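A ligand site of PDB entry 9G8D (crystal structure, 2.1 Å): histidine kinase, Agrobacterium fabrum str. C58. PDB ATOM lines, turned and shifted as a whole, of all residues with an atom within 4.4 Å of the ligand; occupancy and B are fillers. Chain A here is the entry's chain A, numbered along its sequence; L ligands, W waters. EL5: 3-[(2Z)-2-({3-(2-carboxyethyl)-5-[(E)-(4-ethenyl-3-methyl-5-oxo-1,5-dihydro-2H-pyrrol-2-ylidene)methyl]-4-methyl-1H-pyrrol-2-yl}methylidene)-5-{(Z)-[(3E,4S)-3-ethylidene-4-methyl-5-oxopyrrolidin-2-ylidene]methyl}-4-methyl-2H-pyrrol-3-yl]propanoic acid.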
ATOM      1  N   CYS A  13      21.983  -1.554   4.559  1.00  0.00           N
ATOM      2  CA  CYS A  13      21.257  -2.107   3.373  1.00  0.00           C
ATOM      3  C   CYS A  13      19.832  -2.535   3.779  1.00  0.00           C
ATOM      4  O   CYS A  13      18.950  -2.547   2.892  1.00  0.00           O
ATOM      5  CB  CYS A  13      22.028  -3.212   2.665  1.00  0.00           C
ATOM      6  SG  CYS A  13      22.284  -4.727   3.637  1.00  0.00           S
ATOM      7  N   ASP A  14      19.576  -2.789   5.065  1.00  0.00           N
ATOM      8  CA  ASP A  14      18.209  -3.100   5.575  1.00  0.00           C
ATOM      9  C   ASP A  14      17.273  -1.893   5.396  1.00  0.00           C
ATOM     10  O   ASP A  14      16.052  -2.107   5.427  1.00  0.00           O
ATOM     11  CB  ASP A  14      18.226  -3.590   7.019  1.00  0.00           C
ATOM     12  CG  ASP A  14      18.679  -2.562   8.049  1.00  0.00           C
ATOM     13  OD1 ASP A  14      19.283  -1.556   7.649  1.00  0.00           O
ATOM     14  OD2 ASP A  14      18.415  -2.780   9.234  1.00  0.00           O
ATOM     15  N   ILE A  18      15.563   2.018  -1.956  1.00  0.00           N
ATOM     16  CA  ILE A  18      15.707   1.404  -3.316  1.00  0.00           C
ATOM     17  C   ILE A  18      14.597   1.893  -4.252  1.00  0.00           C
ATOM     18  O   ILE A  18      14.721   1.682  -5.477  1.00  0.00           O
ATOM     19  CB  ILE A  18      15.748  -0.135  -3.211  1.00  0.00           C
ATOM     20  CG1 ILE A  18      14.515  -0.706  -2.508  1.00  0.00           C
ATOM     21  CG2 ILE A  18      17.041  -0.557  -2.527  1.00  0.00           C
ATOM     22  CD1 ILE A  18      14.316  -2.193  -2.721  1.00  0.00           C
ATOM     23  N   TYR A 165      10.368 -19.766  -4.802  1.00  0.00           N
ATOM     24  CA  TYR A 165      10.534 -19.612  -3.336  1.00  0.00           C
ATOM     25  C   TYR A 165       9.147 -19.545  -2.713  1.00  0.00           C
ATOM     26  O   TYR A 165       8.304 -18.811  -3.239  1.00  0.00           O
ATOM     27  CB  TYR A 165      11.303 -18.340  -2.962  1.00  0.00           C
ATOM     28  CG  TYR A 165      12.447 -17.962  -3.846  1.00  0.00           C
ATOM     29  CD1 TYR A 165      13.383 -18.900  -4.256  1.00  0.00           C
ATOM     30  CD2 TYR A 165      12.643 -16.651  -4.224  1.00  0.00           C
ATOM     31  CE1 TYR A 165      14.461 -18.542  -5.068  1.00  0.00           C
ATOM     32  CE2 TYR A 165      13.705 -16.266  -5.029  1.00  0.00           C
ATOM     33  CZ  TYR A 165      14.606 -17.217  -5.456  1.00  0.00           C
ATOM     34  OH  TYR A 165      15.661 -16.852  -6.239  1.00  0.00           O
ATOM     35  N   PHE A 187      20.025 -25.337  -5.971  1.00  0.00           N
ATOM     36  CA  PHE A 187      19.579 -24.621  -4.745  1.00  0.00           C
ATOM     37  C   PHE A 187      18.287 -25.249  -4.189  1.00  0.00           C
ATOM     38  O   PHE A 187      17.754 -24.748  -3.200  1.00  0.00           O
ATOM     39  CB  PHE A 187      19.386 -23.134  -5.036  1.00  0.00           C
ATOM     40  CG  PHE A 187      20.628 -22.407  -5.508  1.00  0.00           C
ATOM     41  CD1 PHE A 187      21.793 -22.405  -4.750  1.00  0.00           C
ATOM     42  CD2 PHE A 187      20.611 -21.676  -6.687  1.00  0.00           C
ATOM     43  CE1 PHE A 187      22.913 -21.711  -5.174  1.00  0.00           C
ATOM     44  CE2 PHE A 187      21.744 -20.978  -7.116  1.00  0.00           C
ATOM     45  CZ  PHE A 187      22.893 -21.010  -6.366  1.00  0.00           C
ATOM     46  N   GLN A 190      17.065 -25.494  -0.436  1.00  0.00           N
ATOM     47  CA  GLN A 190      17.830 -24.450   0.293  1.00  0.00           C
ATOM     48  C   GLN A 190      16.855 -23.408   0.873  1.00  0.00           C
ATOM     49  O   GLN A 190      15.765 -23.235   0.306  1.00  0.00           O
ATOM     50  CB  GLN A 190      18.840 -23.791  -0.638  1.00  0.00           C
ATOM     51  CG  GLN A 190      19.839 -22.895   0.069  1.00  0.00           C
ATOM     52  CD  GLN A 190      21.104 -22.687  -0.724  1.00  0.00           C
ATOM     53  OE1 GLN A 190      21.558 -23.579  -1.432  1.00  0.00           O
ATOM     54  NE2 GLN A 190      21.683 -21.507  -0.600  1.00  0.00           N
ATOM     55  N   9IJ A 192      16.923 -19.240   2.508  1.00  0.00           N
ATOM     56  CA  9IJ A 192      17.658 -17.991   2.714  1.00  0.00           C
ATOM     57  C   9IJ A 192      17.027 -17.181   3.840  1.00  0.00           C
ATOM     58  CB  9IJ A 192      17.867 -17.158   1.448  1.00  0.00           C
ATOM     59  CG  9IJ A 192      16.637 -16.914   0.605  1.00  0.00           C
ATOM     60  CD1 9IJ A 192      15.871 -15.771   0.852  1.00  0.00           C
ATOM     61  CD2 9IJ A 192      16.301 -17.784  -0.432  1.00  0.00           C
ATOM     62  CE1 9IJ A 192      14.737 -15.517   0.068  1.00  0.00           C
ATOM     63  CE2 9IJ A 192      15.169 -17.514  -1.198  1.00  0.00           C
ATOM     64  CZ  9IJ A 192      14.395 -16.394  -0.952  1.00  0.00           C
ATOM     65  C01 9IJ A 192      17.006 -18.855  -0.646  1.00  0.00           C
ATOM     66  N01 9IJ A 192      17.637 -19.847  -0.735  1.00  0.00           N
ATOM     67  O   9IJ A 192      15.620 -17.220   3.783  1.00  0.00           O
ATOM     68  N   SER A 195      16.434 -11.428   5.974  1.00  0.00           N
ATOM     69  CA  SER A 195      17.288 -10.223   5.777  1.00  0.00           C
ATOM     70  C   SER A 195      17.828 -10.157   4.342  1.00  0.00           C
ATOM     71  O   SER A 195      18.224  -9.064   3.935  1.00  0.00           O
ATOM     72  CB  SER A 195      18.401 -10.183   6.785  1.00  0.00           C
ATOM     73  OG  SER A 195      19.257 -11.299   6.636  1.00  0.00           O
ATOM     74  N   ASP A 196      17.841 -11.278   3.607  1.00  0.00           N
ATOM     75  CA  ASP A 196      18.288 -11.350   2.195  1.00  0.00           C
ATOM     76  C   ASP A 196      17.361 -10.542   1.298  1.00  0.00           C
ATOM     77  O   ASP A 196      17.798 -10.113   0.205  1.00  0.00           O
ATOM     78  CB  ASP A 196      18.408 -12.800   1.715  1.00  0.00           C
ATOM     79  CG  ASP A 196      19.748 -13.434   2.026  1.00  0.00           C
ATOM     80  OD1 ASP A 196      20.491 -12.861   2.839  1.00  0.00           O
ATOM     81  OD2 ASP A 196      20.028 -14.490   1.452  1.00  0.00           O
ATOM     82  N   ILE A 197      16.104 -10.349   1.711  1.00  0.00           N
ATOM     83  CA  ILE A 197      15.157  -9.483   0.970  1.00  0.00           C
ATOM     84  C   ILE A 197      14.604  -8.449   1.946  1.00  0.00           C
ATOM     85  O   ILE A 197      13.682  -8.751   2.697  1.00  0.00           O
ATOM     86  CB  ILE A 197      14.039 -10.290   0.274  1.00  0.00           C
ATOM     87  CG1 ILE A 197      14.612 -11.378  -0.628  1.00  0.00           C
ATOM     88  CG2 ILE A 197      13.130  -9.348  -0.502  1.00  0.00           C
ATOM     89  CD1 ILE A 197      13.559 -12.252  -1.252  1.00  0.00           C
ATOM     90  N   PRO A 198      15.148  -7.211   1.947  1.00  0.00           N
ATOM     91  CA  PRO A 198      14.726  -6.178   2.886  1.00  0.00           C
ATOM     92  C   PRO A 198      13.267  -5.752   2.685  1.00  0.00           C
ATOM     93  O   PRO A 198      12.713  -5.987   1.626  1.00  0.00           O
ATOM     94  CB  PRO A 198      15.700  -5.015   2.607  1.00  0.00           C
ATOM     95  CG  PRO A 198      16.179  -5.234   1.199  1.00  0.00           C
ATOM     96  CD  PRO A 198      16.208  -6.745   1.039  1.00  0.00           C
ATOM     97  N   ALA A 201      12.148  -3.948  -0.495  1.00  0.00           N
ATOM     98  CA  ALA A 201      12.159  -4.883  -1.651  1.00  0.00           C
ATOM     99  C   ALA A 201      10.880  -5.723  -1.605  1.00  0.00           C
ATOM    100  O   ALA A 201      10.230  -5.851  -2.660  1.00  0.00           O
ATOM    101  CB  ALA A 201      13.412  -5.722  -1.664  1.00  0.00           C
ATOM    102  N   TYR A 205       7.965  -5.982  -4.382  1.00  0.00           N
ATOM    103  CA  TYR A 205       7.573  -7.293  -4.958  1.00  0.00           C
ATOM    104  C   TYR A 205       6.043  -7.449  -4.855  1.00  0.00           C
ATOM    105  O   TYR A 205       5.427  -7.982  -5.791  1.00  0.00           O
ATOM    106  CB  TYR A 205       8.307  -8.461  -4.292  1.00  0.00           C
ATOM    107  CG  TYR A 205       9.746  -8.645  -4.710  1.00  0.00           C
ATOM    108  CD1 TYR A 205      10.111  -8.745  -6.035  1.00  0.00           C
ATOM    109  CD2 TYR A 205      10.752  -8.715  -3.762  1.00  0.00           C
ATOM    110  CE1 TYR A 205      11.431  -8.901  -6.423  1.00  0.00           C
ATOM    111  CE2 TYR A 205      12.082  -8.868  -4.121  1.00  0.00           C
ATOM    112  CZ  TYR A 205      12.428  -8.969  -5.453  1.00  0.00           C
ATOM    113  OH  TYR A 205      13.744  -9.118  -5.805  1.00  0.00           O
ATOM    114  N   ARG A 211       9.584  -7.933 -11.652  1.00  0.00           N
ATOM    115  CA  ARG A 211      10.827  -7.175 -11.404  1.00  0.00           C
ATOM    116  C   ARG A 211      11.840  -7.656 -12.455  1.00  0.00           C
ATOM    117  O   ARG A 211      12.135  -8.888 -12.475  1.00  0.00           O
ATOM    118  CB  ARG A 211      11.292  -7.390  -9.967  1.00  0.00           C
ATOM    119  CG  ARG A 211      12.626  -6.721  -9.625  1.00  0.00           C
ATOM    120  CD  ARG A 211      12.672  -5.268 -10.036  1.00  0.00           C
ATOM    121  NE  ARG A 211      13.826  -4.593  -9.465  1.00  0.00           N
ATOM    122  CZ  ARG A 211      14.320  -3.437  -9.893  1.00  0.00           C
ATOM    123  NH1 ARG A 211      13.804  -2.811 -10.939  1.00  0.00           N
ATOM    124  NH2 ARG A 211      15.358  -2.906  -9.264  1.00  0.00           N
ATOM    125  N   ILE A 213      15.689  -7.323 -14.181  1.00  0.00           N
ATOM    126  CA  ILE A 213      17.116  -6.912 -14.150  1.00  0.00           C
ATOM    127  C   ILE A 213      17.752  -7.418 -15.449  1.00  0.00           C
ATOM    128  O   ILE A 213      17.937  -8.635 -15.578  1.00  0.00           O
ATOM    129  CB  ILE A 213      17.832  -7.432 -12.888  1.00  0.00           C
ATOM    130  CG1 ILE A 213      17.151  -6.939 -11.609  1.00  0.00           C
ATOM    131  CG2 ILE A 213      19.312  -7.070 -12.930  1.00  0.00           C
ATOM    132  CD1 ILE A 213      17.700  -7.543 -10.337  1.00  0.00           C
ATOM    133  N   ARG A 242      13.605   1.024 -13.113  1.00  0.00           N
ATOM    134  CA  ARG A 242      14.259   1.385 -11.830  1.00  0.00           C
ATOM    135  C   ARG A 242      15.546   0.583 -11.656  1.00  0.00           C
ATOM    136  O   ARG A 242      15.496  -0.666 -11.807  1.00  0.00           O
ATOM    137  CB  ARG A 242      13.312   1.136 -10.643  1.00  0.00           C
ATOM    138  CG  ARG A 242      13.922   1.438  -9.286  1.00  0.00           C
ATOM    139  CD  ARG A 242      12.856   1.407  -8.202  1.00  0.00           C
ATOM    140  NE  ARG A 242      12.121   0.159  -8.292  1.00  0.00           N
ATOM    141  CZ  ARG A 242      12.460  -0.973  -7.696  1.00  0.00           C
ATOM    142  NH1 ARG A 242      13.522  -1.028  -6.905  1.00  0.00           N
ATOM    143  NH2 ARG A 242      11.722  -2.058  -7.875  1.00  0.00           N
ATOM    144  N   VAL A 244      19.001  -1.078  -9.699  1.00  0.00           N
ATOM    145  CA  VAL A 244      19.084  -2.186  -8.697  1.00  0.00           C
ATOM    146  C   VAL A 244      20.115  -1.803  -7.634  1.00  0.00           C
ATOM    147  O   VAL A 244      21.178  -1.270  -8.010  1.00  0.00           O
ATOM    148  CB  VAL A 244      19.476  -3.505  -9.372  1.00  0.00           C
ATOM    149  CG1 VAL A 244      19.460  -4.664  -8.379  1.00  0.00           C
ATOM    150  CG2 VAL A 244      18.567  -3.807 -10.553  1.00  0.00           C
ATOM    151  N   SER A 245      19.819  -2.110  -6.372  1.00  0.00           N
ATOM    152  CA  SER A 245      20.798  -1.977  -5.253  1.00  0.00           C
ATOM    153  C   SER A 245      22.146  -2.571  -5.674  1.00  0.00           C
ATOM    154  O   SER A 245      22.187  -3.688  -6.194  1.00  0.00           O
ATOM    155  CB  SER A 245      20.313  -2.637  -4.003  1.00  0.00           C
ATOM    156  OG  SER A 245      21.377  -2.783  -3.080  1.00  0.00           O
ATOM    157  N   ILE A 247      24.150  -3.721  -3.606  1.00  0.00           N
ATOM    158  CA  ILE A 247      24.217  -4.921  -2.717  1.00  0.00           C
ATOM    159  C   ILE A 247      23.766  -6.123  -3.538  1.00  0.00           C
ATOM    160  O   ILE A 247      24.549  -7.089  -3.668  1.00  0.00           O
ATOM    161  CB  ILE A 247      23.353  -4.736  -1.450  1.00  0.00           C
ATOM    162  CG1 ILE A 247      23.793  -3.526  -0.630  1.00  0.00           C
ATOM    163  CG2 ILE A 247      23.351  -6.008  -0.616  1.00  0.00           C
ATOM    164  CD1 ILE A 247      25.224  -3.594  -0.145  1.00  0.00           C
ATOM    165  N   HIS A 248      22.567  -6.063  -4.098  1.00  0.00           N
ATOM    166  CA  HIS A 248      21.960  -7.178  -4.863  1.00  0.00           C
ATOM    167  C   HIS A 248      22.768  -7.439  -6.136  1.00  0.00           C
ATOM    168  O   HIS A 248      22.962  -8.621  -6.475  1.00  0.00           O
ATOM    169  CB  HIS A 248      20.476  -6.941  -5.155  1.00  0.00           C
ATOM    170  CG  HIS A 248      19.883  -8.132  -5.824  1.00  0.00           C
ATOM    171  ND1 HIS A 248      19.955  -9.389  -5.255  1.00  0.00           N
ATOM    172  CD2 HIS A 248      19.265  -8.289  -7.017  1.00  0.00           C
ATOM    173  CE1 HIS A 248      19.368 -10.262  -6.044  1.00  0.00           C
ATOM    174  NE2 HIS A 248      18.942  -9.621  -7.135  1.00  0.00           N
ATOM    175  N   TYR A 251      25.730  -9.466  -5.139  1.00  0.00           N
ATOM    176  CA  TYR A 251      25.208 -10.827  -4.821  1.00  0.00           C
ATOM    177  C   TYR A 251      25.086 -11.635  -6.137  1.00  0.00           C
ATOM    178  O   TYR A 251      25.657 -12.744  -6.240  1.00  0.00           O
ATOM    179  CB  TYR A 251      23.876 -10.745  -4.060  1.00  0.00           C
ATOM    180  CG  TYR A 251      23.558 -11.993  -3.274  1.00  0.00           C
ATOM    181  CD1 TYR A 251      23.311 -13.190  -3.923  1.00  0.00           C
ATOM    182  CD2 TYR A 251      23.554 -11.999  -1.888  1.00  0.00           C
ATOM    183  CE1 TYR A 251      23.038 -14.354  -3.221  1.00  0.00           C
ATOM    184  CE2 TYR A 251      23.273 -13.147  -1.171  1.00  0.00           C
ATOM    185  CZ  TYR A 251      23.023 -14.338  -1.841  1.00  0.00           C
ATOM    186  OH  TYR A 251      22.799 -15.483  -1.161  1.00  0.00           O
ATOM    187  N   MET A 255      27.252 -14.906  -7.754  1.00  0.00           N
ATOM    188  CA  MET A 255      26.607 -16.178  -8.202  1.00  0.00           C
ATOM    189  C   MET A 255      27.034 -16.528  -9.638  1.00  0.00           C
ATOM    190  O   MET A 255      27.030 -17.727  -9.958  1.00  0.00           O
ATOM    191  CB  MET A 255      25.080 -16.068  -8.141  1.00  0.00           C
ATOM    192  CG  MET A 255      24.563 -15.972  -6.720  1.00  0.00           C
ATOM    193  SD  MET A 255      22.789 -15.696  -6.725  1.00  0.00           S
ATOM    194  CE  MET A 255      22.202 -17.307  -7.222  1.00  0.00           C
ATOM    195  N   SER A 260      17.894 -11.161 -14.427  1.00  0.00           N
ATOM    196  CA  SER A 260      16.790 -11.830 -13.703  1.00  0.00           C
ATOM    197  C   SER A 260      15.454 -11.227 -14.105  1.00  0.00           C
ATOM    198  O   SER A 260      15.412 -10.073 -14.584  1.00  0.00           O
ATOM    199  CB  SER A 260      17.012 -11.792 -12.212  1.00  0.00           C
ATOM    200  OG  SER A 260      16.853 -10.478 -11.679  1.00  0.00           O
ATOM    201  N   LEU A 274       7.997 -16.047  -4.924  1.00  0.00           N
ATOM    202  CA  LEU A 274       8.416 -15.537  -6.251  1.00  0.00           C
ATOM    203  C   LEU A 274       8.635 -16.714  -7.183  1.00  0.00           C
ATOM    204  O   LEU A 274       9.100 -17.771  -6.716  1.00  0.00           O
ATOM    205  CB  LEU A 274       9.723 -14.752  -6.095  1.00  0.00           C
ATOM    206  CG  LEU A 274       9.680 -13.517  -5.217  1.00  0.00           C
ATOM    207  CD1 LEU A 274      11.080 -12.928  -5.094  1.00  0.00           C
ATOM    208  CD2 LEU A 274       8.714 -12.473  -5.773  1.00  0.00           C
ATOM    209  N   ALA A 276      11.367 -16.973  -9.658  1.00  0.00           N
ATOM    210  CA  ALA A 276      12.639 -16.262  -9.888  1.00  0.00           C
ATOM    211  C   ALA A 276      13.329 -16.861 -11.108  1.00  0.00           C
ATOM    212  O   ALA A 276      13.656 -18.073 -11.074  1.00  0.00           O
ATOM    213  CB  ALA A 276      13.499 -16.336  -8.659  1.00  0.00           C
ATOM    214  N   HIS A 278      16.626 -16.651 -13.456  1.00  0.00           N
ATOM    215  CA  HIS A 278      18.054 -16.239 -13.458  1.00  0.00           C
ATOM    216  C   HIS A 278      18.719 -16.646 -14.773  1.00  0.00           C
ATOM    217  O   HIS A 278      18.540 -17.811 -15.203  1.00  0.00           O
ATOM    218  CB  HIS A 278      18.797 -16.855 -12.275  1.00  0.00           C
ATOM    219  CG  HIS A 278      18.436 -16.309 -10.948  1.00  0.00           C
ATOM    220  ND1 HIS A 278      18.995 -16.793  -9.791  1.00  0.00           N
ATOM    221  CD2 HIS A 278      17.584 -15.316 -10.577  1.00  0.00           C
ATOM    222  CE1 HIS A 278      18.516 -16.110  -8.761  1.00  0.00           C
ATOM    223  NE2 HIS A 278      17.655 -15.208  -9.220  1.00  0.00           N
ATOM    224  N   ARG A 456      29.269 -12.443   2.776  1.00  0.00           N
ATOM    225  CA  ARG A 456      27.845 -12.227   3.144  1.00  0.00           C
ATOM    226  C   ARG A 456      26.943 -12.376   1.906  1.00  0.00           C
ATOM    227  O   ARG A 456      25.820 -12.897   2.063  1.00  0.00           O
ATOM    228  CB  ARG A 456      27.615 -10.864   3.800  1.00  0.00           C
ATOM    229  CG  ARG A 456      26.158 -10.538   4.114  1.00  0.00           C
ATOM    230  CD  ARG A 456      25.476 -11.575   4.999  1.00  0.00           C
ATOM    231  NE  ARG A 456      24.064 -11.308   5.234  1.00  0.00           N
ATOM    232  CZ  ARG A 456      23.043 -11.734   4.474  1.00  0.00           C
ATOM    233  NH1 ARG A 456      23.255 -12.444   3.391  1.00  0.00           N
ATOM    234  NH2 ARG A 456      21.799 -11.429   4.826  1.00  0.00           N
ATOM    235  N   LEU A 457      27.404 -11.963   0.723  1.00  0.00           N
ATOM    236  CA  LEU A 457      26.536 -11.874  -0.491  1.00  0.00           C
ATOM    237  C   LEU A 457      26.765 -13.120  -1.348  1.00  0.00           C
ATOM    238  O   LEU A 457      27.050 -12.969  -2.544  1.00  0.00           O
ATOM    239  CB  LEU A 457      26.837 -10.579  -1.240  1.00  0.00           C
ATOM    240  CG  LEU A 457      26.726  -9.281  -0.425  1.00  0.00           C
ATOM    241  CD1 LEU A 457      27.102  -8.088  -1.297  1.00  0.00           C
ATOM    242  CD2 LEU A 457      25.331  -9.083   0.160  1.00  0.00           C
ATOM    243  N   PRO A 459      25.179 -17.431  -1.777  1.00  0.00           N
ATOM    244  CA  PRO A 459      24.203 -18.429  -1.325  1.00  0.00           C
ATOM    245  C   PRO A 459      24.727 -19.282  -0.159  1.00  0.00           C
ATOM    246  O   PRO A 459      23.937 -19.632   0.683  1.00  0.00           O
ATOM    247  CB  PRO A 459      23.982 -19.252  -2.600  1.00  0.00           C
ATOM    248  CG  PRO A 459      24.170 -18.243  -3.704  1.00  0.00           C
ATOM    249  CD  PRO A 459      25.376 -17.462  -3.242  1.00  0.00           C
ATOM    250  N   SER A 462      24.367 -17.100   2.999  1.00  0.00           N
ATOM    251  CA  SER A 462      22.935 -16.967   3.203  1.00  0.00           C
ATOM    252  C   SER A 462      22.378 -18.217   3.911  1.00  0.00           C
ATOM    253  O   SER A 462      21.655 -18.069   4.889  1.00  0.00           O
ATOM    254  CB  SER A 462      22.213 -16.717   1.903  1.00  0.00           C
ATOM    255  OG  SER A 462      22.375 -15.393   1.440  1.00  0.00           O
HETATM  256  C1A EL5 L   1      21.227  -9.377   0.761  1.00  0.00           C
HETATM  257  C1B EL5 L   1      18.331  -7.154  -1.690  1.00  0.00           C
HETATM  258  O1B EL5 L   1      15.727  -4.399  -6.764  1.00  0.00           O
HETATM  259  C1C EL5 L   1      17.018 -10.796  -3.550  1.00  0.00           C
HETATM  260  O1C EL5 L   1      16.179 -12.912  -8.120  1.00  0.00           O
HETATM  261  C1D EL5 L   1      19.254 -14.843  -2.339  1.00  0.00           C
HETATM  262  C2A EL5 L   1      21.292  -8.376   1.720  1.00  0.00           C
HETATM  263  C2B EL5 L   1      17.577  -6.276  -2.466  1.00  0.00           C
HETATM  264  O2B EL5 L   1      15.334  -6.311  -7.807  1.00  0.00           O
HETATM  265  C2C EL5 L   1      16.304 -11.934  -3.928  1.00  0.00           C
HETATM  266  O2C EL5 L   1      15.538 -14.162  -6.449  1.00  0.00           O
HETATM  267  C2D EL5 L   1      19.393 -15.570  -3.511  1.00  0.00           C
HETATM  268  C3A EL5 L   1      20.597  -7.236   1.363  1.00  0.00           C
HETATM  269  C3B EL5 L   1      16.885  -7.043  -3.403  1.00  0.00           C
HETATM  270  C3C EL5 L   1      16.920 -13.012  -3.342  1.00  0.00           C
HETATM  271  C3D EL5 L   1      19.888 -16.825  -3.167  1.00  0.00           C
HETATM  272  C4A EL5 L   1      19.978  -7.609   0.166  1.00  0.00           C
HETATM  273  C4B EL5 L   1      17.184  -8.363  -3.118  1.00  0.00           C
HETATM  274  C4C EL5 L   1      18.089 -12.589  -2.695  1.00  0.00           C
HETATM  275  C4D EL5 L   1      20.077 -16.844  -1.780  1.00  0.00           C
HETATM  276  CAA EL5 L   1      20.450  -6.035   2.124  1.00  0.00           C
HETATM  277  CAB EL5 L   1      15.972  -6.563  -4.495  1.00  0.00           C
HETATM  278  CAC EL5 L   1      15.044 -11.993  -4.765  1.00  0.00           C
HETATM  279  CAD EL5 L   1      20.137 -17.877  -4.068  1.00  0.00           C
HETATM  280  CBA EL5 L   1      20.944  -5.749   3.367  1.00  0.00           C
HETATM  281  CBB EL5 L   1      16.670  -6.377  -5.837  1.00  0.00           C
HETATM  282  CBC EL5 L   1      15.194 -11.815  -6.267  1.00  0.00           C
HETATM  283  CBD EL5 L   1      20.393 -19.113  -3.772  1.00  0.00           C
HETATM  284  CGB EL5 L   1      15.844  -5.635  -6.878  1.00  0.00           C
HETATM  285  CGC EL5 L   1      15.673 -13.054  -6.993  1.00  0.00           C
HETATM  286  CHB EL5 L   1      19.090  -6.829  -0.571  1.00  0.00           C
HETATM  287  CHC EL5 L   1      16.763  -9.464  -3.839  1.00  0.00           C
HETATM  288  CHD EL5 L   1      18.785 -13.570  -2.029  1.00  0.00           C
HETATM  289  CMA EL5 L   1      22.346  -8.379   2.782  1.00  0.00           C
HETATM  290  CMB EL5 L   1      17.544  -4.782  -2.349  1.00  0.00           C
HETATM  291  CMC EL5 L   1      16.442 -14.424  -3.454  1.00  0.00           C
HETATM  292  CMD EL5 L   1      19.132 -15.113  -4.923  1.00  0.00           C
HETATM  293  NA  EL5 L   1      20.371  -8.878  -0.202  1.00  0.00           N
HETATM  294  OA  EL5 L   1      21.778 -10.453   0.734  1.00  0.00           O
HETATM  295  NB  EL5 L   1      18.026  -8.439  -2.043  1.00  0.00           N
HETATM  296  NC  EL5 L   1      18.055 -11.218  -2.722  1.00  0.00           N
HETATM  297  ND  EL5 L   1      19.701 -15.623  -1.302  1.00  0.00           N
HETATM  298  OD  EL5 L   1      20.463 -17.744  -1.044  1.00  0.00           O
HETATM  299  O   HOH W   1      20.801 -19.616   1.075  1.00  0.00           O
HETATM  300  O   HOH W   2      18.593  -2.969   0.256  1.00  0.00           O
HETATM  301  O   HOH W   3      14.381 -13.020 -10.249  1.00  0.00           O
HETATM  302  O   HOH W   4      13.308  -3.681  -5.956  1.00  0.00           O
HETATM  303  O   HOH W   5      20.639 -10.179  -2.732  1.00  0.00           O
HETATM  304  O   HOH W   6      17.120  -2.595  -5.566  1.00  0.00           O
HETATM  305  O   HOH W   7      14.913  -8.815  -8.286  1.00  0.00           O
HETATM  306  O   HOH W   8      17.041 -10.808  -8.902  1.00  0.00           O
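SG of Cys 13 is bonded to CBA of the ligand (1.7 Å).
The side-chain hydroxyl (OH) of Tyr 165 lies within hydrogen-bond range of an oxygen (O2C) of the ligand, at 2.7 Å.
NA of the ligand is in hydrogen-bond range of O of Asp 196 (2.9 Å).
A nitrogen (ND) of the ligand lies within hydrogen-bond range of the side-chain carboxylate (OD2) of Asp 196 (3.0 Å).
NE of Arg 211 is in salt-bridge range of O2B of the ligand, at 2.8 Å.
NE2 of His 278 is in hydrogen-bond range of O1C of the ligand, at 2.9 Å.
The side-chain hydroxyl (OH) of Tyr 251 is in hydrogen-bond range of a nitrogen (ND) of the ligand, 3.1 Å away.
O of Leu 274 is in hydrogen-bond range of N of Tyr 165, at 3.0 Å.
The side-chain carboxylate (OD1) of Asp 196 is in salt-bridge range of the guanidinium group (NH2) of Arg 456, 2.8 Å away.
The guanidinium group (NH1) of Arg 211 sits at hydrogen-bond distance from the backbone carbonyl oxygen (O) of Arg 242 (2.9 Å).
The side-chain hydroxyl (OH) of Tyr 251 sits at hydrogen-bond distance from the side-chain hydroxyl (OG) of Ser 462 (2.6 Å).
The side-chain hydroxyl (OG) of Ser 245 sits at hydrogen-bond distance from the backbone NH (N) of Ile 247, 3.0 Å away.
The guanidinium group of Arg 456 lies within hydrogen-bond range of the side-chain hydroxyl of Ser 195 (3.1 Å).
The backbone NH (N) of Ser 260 is in hydrogen-bond range of the backbone carbonyl oxygen (O) of Ile 213 (2.8 Å).
O of Pro 459 lies within hydrogen-bond range of NE2 of Gln 190, at 3.2 Å.
Asp 14 touches the ligand (N to CBA, 3.7 Å).
Phe 187 touches the ligand (CD1 to CBD, 3.7 Å).
Gln 190 touches the ligand (NE2 to OD, 3.98 Å).
9IJ 192 touches the ligand (N01 to OD, 3.5 Å).
Ser 195 touches the ligand (O to C2A, 3.8 Å).
Ile 197 touches the ligand.
Pro 198 touches the ligand (CD to CHB, 3.3 Å).
Ala 201 touches the ligand (CB to CAB, 3.9 Å).
OH of Tyr 205 touches CBC of the ligand, 3.1 Å away.
CD1 of Ile 213 touches O2B of the ligand, 3.7 Å away.
Ser 245 touches the ligand.
Ile 247 touches the ligand (CG2 to C3A, 3.6 Å).
His 248 touches the ligand (CD2 to CBB, 3.4 Å).
CE of Met 255 touches CAD of the ligand (3.8 Å).
Ala 276 touches the ligand (CB to O2C, 3.7 Å).
Arg 456 touches the ligand.
CD2 of Leu 457 touches OA of the ligand, 3.9 Å away.
Pro 459 touches the ligand (CB to CBD, 3.8 Å).
CB of Ser 462 touches OD of the ligand, 3.6 Å away.
Within 4 Å of the ligand: Cys 13, Asp 14, Tyr 165, Phe 187, Gln 190, 9IJ 192, Ser 195, Asp 196, Ile 197, Pro 198, Ala 201, Tyr 205, Arg 211, Ile 213, Ser 245, Ile 247, His 248, Tyr 251, Met 255, Ala 276, His 278, Arg 456, Leu 457, Pro 459 and Ser 462.
Water W8 lies within hydrogen-bond range of O1C of the ligand (2.4 Å), OG of Ser 260 (2.8 Å) and NE2 of His 248 (2.9 Å).
Water W6 lies within hydrogen-bond range of O1B of the ligand (2.6 Å) and N of Ser 245 (2.9 Å).
Water W7 lies within hydrogen-bond range of O2B of the ligand (2.6 Å) and OH of Tyr 205 (2.8 Å).
Water W4 lies within hydrogen-bond range of an oxygen (O1B) of the ligand (2.6 Å) and the guanidinium group (NH1) of Arg 242 (2.8 Å).
Water W5 lies within hydrogen-bond range of ND1 of His 248 (2.7 Å) and NC of the ligand (2.8 Å).
Water W1 lies within hydrogen-bond range of the side-chain amide nitrogen (NE2) of Gln 190 (2.7 Å), an oxygen (OD) of the ligand (2.8 Å) and the backbone carbonyl oxygen (O) of Pro 459 (3.2 Å).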
